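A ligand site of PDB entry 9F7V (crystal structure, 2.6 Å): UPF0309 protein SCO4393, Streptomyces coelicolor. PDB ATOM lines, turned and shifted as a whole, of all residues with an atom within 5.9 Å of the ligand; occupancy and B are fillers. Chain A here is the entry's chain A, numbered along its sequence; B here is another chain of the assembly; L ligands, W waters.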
ATOM      1  N   ALA A  51     -25.188  -3.419  12.391  1.00  0.00           N
ATOM      2  CA  ALA A  51     -24.766  -2.098  12.835  1.00  0.00           C
ATOM      3  C   ALA A  51     -23.253  -2.053  12.975  1.00  0.00           C
ATOM      4  O   ALA A  51     -22.614  -3.032  13.347  1.00  0.00           O
ATOM      5  CB  ALA A  51     -25.418  -1.746  14.180  1.00  0.00           C
ATOM      6  N   GLY A  52     -22.687  -0.892  12.664  1.00  0.00           N
ATOM      7  CA  GLY A  52     -21.268  -0.692  12.889  1.00  0.00           C
ATOM      8  C   GLY A  52     -20.484  -1.710  12.089  1.00  0.00           C
ATOM      9  O   GLY A  52     -20.727  -1.915  10.902  1.00  0.00           O
ATOM     10  N   HIS A  53     -19.508  -2.354  12.737  1.00  0.00           N
ATOM     11  CA  HIS A  53     -18.704  -3.329  12.017  1.00  0.00           C
ATOM     12  C   HIS A  53     -19.489  -4.586  11.661  1.00  0.00           C
ATOM     13  O   HIS A  53     -19.073  -5.343  10.784  1.00  0.00           O
ATOM     14  CB  HIS A  53     -17.452  -3.704  12.810  1.00  0.00           C
ATOM     15  CG  HIS A  53     -16.494  -2.560  12.986  1.00  0.00           C
ATOM     16  ND1 HIS A  53     -16.527  -1.730  14.084  1.00  0.00           N
ATOM     17  CD2 HIS A  53     -15.532  -2.073  12.175  1.00  0.00           C
ATOM     18  CE1 HIS A  53     -15.601  -0.803  13.954  1.00  0.00           C
ATOM     19  NE2 HIS A  53     -14.986  -0.981  12.805  1.00  0.00           N
ATOM     20  N   SER A  54     -20.626  -4.824  12.319  1.00  0.00           N
ATOM     21  CA  SER A  54     -21.486  -5.929  11.910  1.00  0.00           C
ATOM     22  C   SER A  54     -22.156  -5.645  10.573  1.00  0.00           C
ATOM     23  O   SER A  54     -22.571  -6.585   9.878  1.00  0.00           O
ATOM     24  CB  SER A  54     -22.548  -6.201  12.972  1.00  0.00           C
ATOM     25  OG  SER A  54     -22.034  -6.994  14.035  1.00  0.00           O
ATOM     26  N   ILE A  82     -18.769   2.425   9.814  1.00  0.00           N
ATOM     27  CA  ILE A  82     -18.298   3.387  10.796  1.00  0.00           C
ATOM     28  C   ILE A  82     -18.045   4.741  10.141  1.00  0.00           C
ATOM     29  O   ILE A  82     -17.305   5.566  10.676  1.00  0.00           O
ATOM     30  CB  ILE A  82     -17.057   2.873  11.544  1.00  0.00           C
ATOM     31  CG1 ILE A  82     -16.000   2.326  10.583  1.00  0.00           C
ATOM     32  CG2 ILE A  82     -17.451   1.766  12.515  1.00  0.00           C
ATOM     33  CD1 ILE A  82     -15.321   3.382   9.745  1.00  0.00           C
ATOM     34  N   GLY A  90     -22.391   6.397  16.036  1.00  0.00           N
ATOM     35  CA  GLY A  90     -22.889   5.078  15.658  1.00  0.00           C
ATOM     36  C   GLY A  90     -23.204   4.216  16.857  1.00  0.00           C
ATOM     37  O   GLY A  90     -24.242   3.550  16.905  1.00  0.00           O
ATOM     38  N   SER A  91     -22.325   4.241  17.860  1.00  0.00           N
ATOM     39  CA  SER A  91     -22.565   3.486  19.086  1.00  0.00           C
ATOM     40  C   SER A  91     -23.800   3.994  19.812  1.00  0.00           C
ATOM     41  O   SER A  91     -24.590   3.200  20.346  1.00  0.00           O
ATOM     42  CB  SER A  91     -21.329   3.568  19.994  1.00  0.00           C
ATOM     43  OG  SER A  91     -20.144   3.368  19.254  1.00  0.00           O
ATOM     44  N   GLU A  94     -27.244   2.831  18.368  1.00  0.00           N
ATOM     45  CA  GLU A  94     -27.671   1.470  18.700  1.00  0.00           C
ATOM     46  C   GLU A  94     -28.530   1.412  19.949  1.00  0.00           C
ATOM     47  O   GLU A  94     -29.125   0.356  20.216  1.00  0.00           O
ATOM     48  CB  GLU A  94     -26.446   0.569  18.853  1.00  0.00           C
ATOM     49  CG  GLU A  94     -25.702   0.403  17.541  1.00  0.00           C
ATOM     50  CD  GLU A  94     -24.373  -0.263  17.719  1.00  0.00           C
ATOM     51  OE1 GLU A  94     -24.249  -1.088  18.656  1.00  0.00           O
ATOM     52  OE2 GLU A  94     -23.456   0.042  16.931  1.00  0.00           O
ATOM     53  N   ILE A 118     -27.127  -9.319  11.715  1.00  0.00           N
ATOM     54  CA  ILE A 118     -25.820  -9.594  12.289  1.00  0.00           C
ATOM     55  C   ILE A 118     -25.601  -8.653  13.467  1.00  0.00           C
ATOM     56  O   ILE A 118     -25.629  -7.429  13.303  1.00  0.00           O
ATOM     57  CB  ILE A 118     -24.694  -9.423  11.251  1.00  0.00           C
ATOM     58  CG1 ILE A 118     -24.905 -10.354  10.049  1.00  0.00           C
ATOM     59  CG2 ILE A 118     -23.339  -9.709  11.890  1.00  0.00           C
ATOM     60  CD1 ILE A 118     -24.984  -9.615   8.732  1.00  0.00           C
ATOM     61  N   SER A 119     -25.405  -9.229  14.648  1.00  0.00           N
ATOM     62  CA  SER A 119     -25.050  -8.479  15.849  1.00  0.00           C
ATOM     63  C   SER A 119     -24.254  -9.413  16.736  1.00  0.00           C
ATOM     64  O   SER A 119     -24.791 -10.412  17.227  1.00  0.00           O
ATOM     65  CB  SER A 119     -26.283  -7.957  16.565  1.00  0.00           C
ATOM     66  OG  SER A 119     -25.930  -7.293  17.762  1.00  0.00           O
ATOM     67  N   LEU A 120     -22.973  -9.085  16.960  1.00  0.00           N
ATOM     68  CA  LEU A 120     -22.126  -9.955  17.762  1.00  0.00           C
ATOM     69  C   LEU A 120     -22.659 -10.090  19.185  1.00  0.00           C
ATOM     70  O   LEU A 120     -22.846 -11.202  19.690  1.00  0.00           O
ATOM     71  CB  LEU A 120     -20.691  -9.439  17.775  1.00  0.00           C
ATOM     72  CG  LEU A 120     -19.669 -10.453  18.298  1.00  0.00           C
ATOM     73  CD1 LEU A 120     -19.520 -11.622  17.322  1.00  0.00           C
ATOM     74  CD2 LEU A 120     -18.325  -9.819  18.596  1.00  0.00           C
ATOM     75  N   SER A 121     -22.906  -8.956  19.848  1.00  0.00           N
ATOM     76  CA  SER A 121     -23.374  -8.992  21.220  1.00  0.00           C
ATOM     77  C   SER A 121     -24.849  -9.354  21.332  1.00  0.00           C
ATOM     78  O   SER A 121     -25.253 -10.015  22.295  1.00  0.00           O
ATOM     79  CB  SER A 121     -23.110  -7.649  21.897  1.00  0.00           C
ATOM     80  OG  SER A 121     -23.915  -6.617  21.348  1.00  0.00           O
ATOM     81  N   GLY A 122     -25.656  -8.955  20.352  1.00  0.00           N
ATOM     82  CA  GLY A 122     -27.094  -9.165  20.426  1.00  0.00           C
ATOM     83  C   GLY A 122     -27.789  -8.519  21.613  1.00  0.00           C
ATOM     84  O   GLY A 122     -28.889  -8.937  21.968  1.00  0.00           O
ATOM     85  N   ASN A 124     -28.021  -4.874  22.376  1.00  0.00           N
ATOM     86  CA  ASN A 124     -28.441  -3.483  22.327  1.00  0.00           C
ATOM     87  C   ASN A 124     -29.869  -3.360  21.789  1.00  0.00           C
ATOM     88  O   ASN A 124     -30.407  -4.275  21.157  1.00  0.00           O
ATOM     89  CB  ASN A 124     -27.495  -2.638  21.471  1.00  0.00           C
ATOM     90  CG  ASN A 124     -26.127  -2.481  22.099  1.00  0.00           C
ATOM     91  OD1 ASN A 124     -26.012  -2.284  23.309  1.00  0.00           O
ATOM     92  ND2 ASN A 124     -25.085  -2.538  21.283  1.00  0.00           N
ATOM     93  N   PRO A 127     -30.568  -3.810  17.489  1.00  0.00           N
ATOM     94  CA  PRO A 127     -30.723  -5.132  16.861  1.00  0.00           C
ATOM     95  C   PRO A 127     -31.838  -5.959  17.478  1.00  0.00           C
ATOM     96  O   PRO A 127     -32.476  -6.751  16.764  1.00  0.00           O
ATOM     97  CB  PRO A 127     -29.344  -5.781  17.061  1.00  0.00           C
ATOM     98  CG  PRO A 127     -28.729  -5.029  18.188  1.00  0.00           C
ATOM     99  CD  PRO A 127     -29.237  -3.630  18.085  1.00  0.00           C
ATOM    100  N   ASP A 179     -14.390  -9.507  21.977  1.00  0.00           N
ATOM    101  CA  ASP A 179     -14.033  -9.429  20.558  1.00  0.00           C
ATOM    102  C   ASP A 179     -12.558  -9.055  20.380  1.00  0.00           C
ATOM    103  O   ASP A 179     -12.210  -8.062  19.738  1.00  0.00           O
ATOM    104  CB  ASP A 179     -14.938  -8.454  19.822  1.00  0.00           C
ATOM    105  CG  ASP A 179     -14.901  -8.643  18.318  1.00  0.00           C
ATOM    106  OD1 ASP A 179     -14.267  -9.627  17.878  1.00  0.00           O
ATOM    107  OD2 ASP A 179     -15.489  -7.823  17.594  1.00  0.00           O
ATOM    108  N   TYR B  63     -11.844   2.487  14.624  1.00  0.00           N
ATOM    109  CA  TYR B  63     -12.737   2.582  15.784  1.00  0.00           C
ATOM    110  C   TYR B  63     -13.208   1.200  16.206  1.00  0.00           C
ATOM    111  O   TYR B  63     -14.399   0.932  16.375  1.00  0.00           O
ATOM    112  CB  TYR B  63     -13.922   3.507  15.462  1.00  0.00           C
ATOM    113  CG  TYR B  63     -14.878   3.765  16.609  1.00  0.00           C
ATOM    114  CD1 TYR B  63     -14.425   4.263  17.820  1.00  0.00           C
ATOM    115  CD2 TYR B  63     -16.237   3.518  16.469  1.00  0.00           C
ATOM    116  CE1 TYR B  63     -15.298   4.513  18.861  1.00  0.00           C
ATOM    117  CE2 TYR B  63     -17.112   3.761  17.498  1.00  0.00           C
ATOM    118  CZ  TYR B  63     -16.640   4.257  18.698  1.00  0.00           C
ATOM    119  OH  TYR B  63     -17.509   4.488  19.733  1.00  0.00           O
ATOM    120  N   ARG B  64     -12.241   0.311  16.424  1.00  0.00           N
ATOM    121  CA  ARG B  64     -12.516  -1.118  16.494  1.00  0.00           C
ATOM    122  C   ARG B  64     -12.131  -1.655  17.856  1.00  0.00           C
ATOM    123  O   ARG B  64     -11.043  -1.355  18.369  1.00  0.00           O
ATOM    124  CB  ARG B  64     -11.733  -1.848  15.393  1.00  0.00           C
ATOM    125  CG  ARG B  64     -12.006  -3.328  15.299  1.00  0.00           C
ATOM    126  CD  ARG B  64     -13.386  -3.534  14.679  1.00  0.00           C
ATOM    127  NE  ARG B  64     -13.548  -4.870  14.122  1.00  0.00           N
ATOM    128  CZ  ARG B  64     -14.027  -5.916  14.792  1.00  0.00           C
ATOM    129  NH1 ARG B  64     -14.249  -5.855  16.093  1.00  0.00           N
ATOM    130  NH2 ARG B  64     -14.200  -7.064  14.152  1.00  0.00           N
ATOM    131  N   ALA B  65     -13.023  -2.451  18.448  1.00  0.00           N
ATOM    132  CA  ALA B  65     -12.674  -3.259  19.624  1.00  0.00           C
ATOM    133  C   ALA B  65     -11.389  -4.027  19.375  1.00  0.00           C
ATOM    134  O   ALA B  65     -11.289  -4.801  18.414  1.00  0.00           O
ATOM    135  CB  ALA B  65     -13.811  -4.212  19.959  1.00  0.00           C
ATOM    136  N   LEU B 224      -8.329   0.295  21.811  1.00  0.00           N
ATOM    137  CA  LEU B 224      -9.726   0.480  22.189  1.00  0.00           C
ATOM    138  C   LEU B 224     -10.324  -0.836  22.672  1.00  0.00           C
ATOM    139  O   LEU B 224      -9.867  -1.916  22.322  1.00  0.00           O
ATOM    140  CB  LEU B 224     -10.541   1.011  21.008  1.00  0.00           C
ATOM    141  CG  LEU B 224     -10.049   2.322  20.397  1.00  0.00           C
ATOM    142  CD1 LEU B 224     -10.808   2.646  19.130  1.00  0.00           C
ATOM    143  CD2 LEU B 224     -10.189   3.449  21.406  1.00  0.00           C
ATOM    144  N   ARG B 225     -11.353  -0.720  23.517  1.00  0.00           N
ATOM    145  CA  ARG B 225     -12.134  -1.845  23.979  1.00  0.00           C
ATOM    146  C   ARG B 225     -13.500  -1.856  23.309  1.00  0.00           C
ATOM    147  O   ARG B 225     -13.960  -0.840  22.774  1.00  0.00           O
ATOM    148  CB  ARG B 225     -12.312  -1.784  25.499  1.00  0.00           C
ATOM    149  CG  ARG B 225     -11.053  -2.108  26.276  1.00  0.00           C
ATOM    150  CD  ARG B 225     -11.299  -2.117  27.763  1.00  0.00           C
ATOM    151  NE  ARG B 225     -10.130  -2.582  28.504  1.00  0.00           N
ATOM    152  CZ  ARG B 225      -9.890  -3.844  28.808  1.00  0.00           C
ATOM    153  NH1 ARG B 225     -10.670  -4.825  28.379  1.00  0.00           N
ATOM    154  NH2 ARG B 225      -8.811  -4.140  29.529  1.00  0.00           N
ATOM    155  N   SER B 226     -14.164  -3.003  23.351  1.00  0.00           N
ATOM    156  CA  SER B 226     -15.501  -3.100  22.764  1.00  0.00           C
ATOM    157  C   SER B 226     -16.461  -2.234  23.561  1.00  0.00           C
ATOM    158  O   SER B 226     -16.531  -2.338  24.790  1.00  0.00           O
ATOM    159  CB  SER B 226     -15.972  -4.550  22.753  1.00  0.00           C
ATOM    160  OG  SER B 226     -17.290  -4.659  22.246  1.00  0.00           O
ATOM    161  N   GLY B 227     -17.247  -1.417  22.865  1.00  0.00           N
ATOM    162  CA  GLY B 227     -18.319  -0.680  23.512  1.00  0.00           C
ATOM    163  C   GLY B 227     -19.512  -1.504  23.941  1.00  0.00           C
ATOM    164  O   GLY B 227     -20.418  -0.959  24.572  1.00  0.00           O
ATOM    165  N   ASN B 228     -19.542  -2.803  23.620  1.00  0.00           N
ATOM    166  CA  ASN B 228     -20.648  -3.674  23.991  1.00  0.00           C
ATOM    167  C   ASN B 228     -20.244  -4.631  25.105  1.00  0.00           C
ATOM    168  O   ASN B 228     -20.945  -5.612  25.365  1.00  0.00           O
ATOM    169  CB  ASN B 228     -21.156  -4.422  22.771  1.00  0.00           C
ATOM    170  CG  ASN B 228     -21.652  -3.488  21.692  1.00  0.00           C
ATOM    171  OD1 ASN B 228     -22.360  -2.519  21.962  1.00  0.00           O
ATOM    172  ND2 ASN B 228     -21.249  -3.751  20.446  1.00  0.00           N
ATOM    173  N   HIS B 233     -17.031   2.049  26.579  1.00  0.00           N
ATOM    174  CA  HIS B 233     -17.129   3.428  26.102  1.00  0.00           C
ATOM    175  C   HIS B 233     -16.385   4.389  27.036  1.00  0.00           C
ATOM    176  O   HIS B 233     -15.790   5.368  26.578  1.00  0.00           O
ATOM    177  CB  HIS B 233     -18.584   3.833  25.929  1.00  0.00           C
ATOM    178  CG  HIS B 233     -19.259   3.162  24.771  1.00  0.00           C
ATOM    179  ND1 HIS B 233     -20.438   2.444  24.899  1.00  0.00           N
ATOM    180  CD2 HIS B 233     -18.902   3.060  23.467  1.00  0.00           C
ATOM    181  CE1 HIS B 233     -20.775   1.963  23.720  1.00  0.00           C
ATOM    182  NE2 HIS B 233     -19.863   2.320  22.840  1.00  0.00           N
ATOM    183  N   ASN B 236     -12.746   3.946  26.154  1.00  0.00           N
ATOM    184  CA  ASN B 236     -12.404   4.552  24.864  1.00  0.00           C
ATOM    185  C   ASN B 236     -12.397   6.067  24.951  1.00  0.00           C
ATOM    186  O   ASN B 236     -11.552   6.716  24.308  1.00  0.00           O
ATOM    187  CB  ASN B 236     -13.383   4.106  23.783  1.00  0.00           C
ATOM    188  CG  ASN B 236     -13.281   2.625  23.456  1.00  0.00           C
ATOM    189  OD1 ASN B 236     -12.348   1.947  23.889  1.00  0.00           O
ATOM    190  ND2 ASN B 236     -14.234   2.131  22.689  1.00  0.00           N
HETATM  191  C1  LIG L   1     -18.347  -1.500  16.548  1.00  0.00           C
HETATM  192  C2  LIG L   1     -18.721  -0.343  17.461  1.00  0.00           C
HETATM  193  C3  LIG L   1     -19.664  -0.759  18.521  1.00  0.00           C
HETATM  194  C4  LIG L   1     -20.868  -1.412  17.907  1.00  0.00           C
HETATM  195  C5  LIG L   1     -20.465  -2.639  17.092  1.00  0.00           C
HETATM  196  C6  LIG L   1     -21.713  -3.245  16.501  1.00  0.00           C
HETATM  197  C7  LIG L   1     -16.675  -0.360  19.142  1.00  0.00           C
HETATM  198  C8  LIG L   1     -15.391   0.332  19.636  1.00  0.00           C
HETATM  199  N1  LIG L   1     -17.448   0.257  18.025  1.00  0.00           N
HETATM  200  O1  LIG L   1     -17.525  -2.350  17.240  1.00  0.00           O
HETATM  201  O2  LIG L   1     -20.083   0.409  19.275  1.00  0.00           O
HETATM  202  O3  LIG L   1     -21.763  -1.814  18.932  1.00  0.00           O
HETATM  203  O4  LIG L   1     -19.525  -2.285  16.021  1.00  0.00           O
HETATM  204  O5  LIG L   1     -22.418  -3.848  17.552  1.00  0.00           O
HETATM  205  O6  LIG L   1     -17.033  -1.373  19.646  1.00  0.00           O
HETATM  206  P1  LIG L   1     -22.723  -5.507  17.509  1.00  0.00           P
HETATM  207  O7  LIG L   1     -24.172  -5.700  17.151  1.00  0.00           O
HETATM  208  O8  LIG L   1     -21.860  -6.193  16.466  1.00  0.00           O
HETATM  209  O9  LIG L   1     -22.425  -6.105  18.861  1.00  0.00           O
HETATM  210  O   HOH W   1     -19.338  -6.191  15.509  1.00  0.00           O
HETATM  211  O   HOH W   2     -25.486  -3.735  18.478  1.00  0.00           O
HETATM  212  O   HOH W   3     -25.577  -4.837  14.867  1.00  0.00           O
HETATM  213  O   HOH W   4     -19.871  -6.486  19.728  1.00  0.00           O
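O of Gly 227 of chain B lies close to ND1 of His 233 of chain B (3.4 Å).
OH of Tyr 63 of chain B sits at hydrogen-bond distance from OG of Ser 91 (2.9 Å).
The backbone NH (N) of Arg 225 of chain B lies within hydrogen-bond range of the side-chain amide oxygen (OD1) of Asn 236 of chain B (2.9 Å).
ND2 of Asn 124 lies within hydrogen-bond range of OD1 of Asn 228 of chain B (2.8 Å).
ND2 of Asn 124 is in hydrogen-bond range of OE1 of Glu 94 (3.1 Å).
The backbone NH (N) of Asn 228 of chain B lies close to the side-chain hydroxyl (OG) of Ser 226 of chain B (3.2 Å).
The backbone NH (N) of Gly 122 is in hydrogen-bond range of the side-chain hydroxyl (OG) of Ser 119 (3.1 Å).
Water W1 lies within hydrogen-bond range of O8 of the ligand (2.7 Å) and OG of Ser 54 (3.2 Å).
Water W2 lies within hydrogen-bond range of O7 of the ligand (2.7 Å), OE1 of Glu 94 (2.9 Å) and ND2 of Asn 124 (3.1 Å).
Water W4 bridges an oxygen (O9) of the ligand (2.7 Å) and the side-chain amide nitrogen of Asn 228 of chain B (3.1 Å).
Water W3 lies within hydrogen-bond range of an oxygen (O7) of the ligand, the backbone NH (N) of Ala 51 and the backbone carbonyl oxygen (O) of Ile 118.
OG of Ser 119 lies within hydrogen-bond range of O7 of the ligand, at 2.4 Å.
OE1 of Glu 94 lies within hydrogen-bond range of O3 of the ligand, at 2.6 Å.
An oxygen (O4) of the ligand sits at hydrogen-bond distance from the backbone NH (N) of His 53 (3.3 Å).
An oxygen (O6) of the ligand lies within hydrogen-bond range of the backbone NH of Gly 227 of chain B (3.2 Å).
The backbone NH (N) of Ser 121 is in hydrogen-bond range of an oxygen (O9) of the ligand, at 3.1 Å.
An oxygen (O8) of the ligand sits at hydrogen-bond distance from the backbone NH of Leu 120 (3.1 Å).
ND2 of Asn 228 of chain B lies within hydrogen-bond range of O3 of the ligand (2.5 Å).
ND1 of His 53 sits close to O1 of the ligand, 3.4 Å away.
O9 of the ligand is in hydrogen-bond range of OG of Ser 121 (2.9 Å).
An oxygen (O8) of the ligand sits at hydrogen-bond distance from the side-chain hydroxyl of Ser 54 (2.6 Å).
An oxygen (O2) of the ligand lies within hydrogen-bond range of the side-chain hydroxyl (OG) of Ser 91 (3.0 Å).
Merely in contact with the ligand: Ala 51 (3.3 Å), Tyr 63 of chain B (3.5 Å), Arg 225 of chain B (3.6 Å), Asn 236 of chain B (3.7 Å), Ala 65 of chain B (3.8 Å), Ser 226 of chain B (3.9 Å) and Gly 52 (3.9 Å).
Hydrophobic or aromatic side chains within 4 Å of the ligand: His 53, Leu 120 and Tyr 63 of chain B.
16 residues have an atom within 4 Å of the ligand: Ala 51, Gly 52, His 53, Ser 54, Ser 91, Glu 94, Ser 119, Leu 120, Ser 121, Tyr 63 of chain B, Ala 65 of chain B, Arg 225 of chain B, Ser 226 of chain B, Gly 227 of chain B, Asn 228 of chain B and Asn 236 of chain B.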
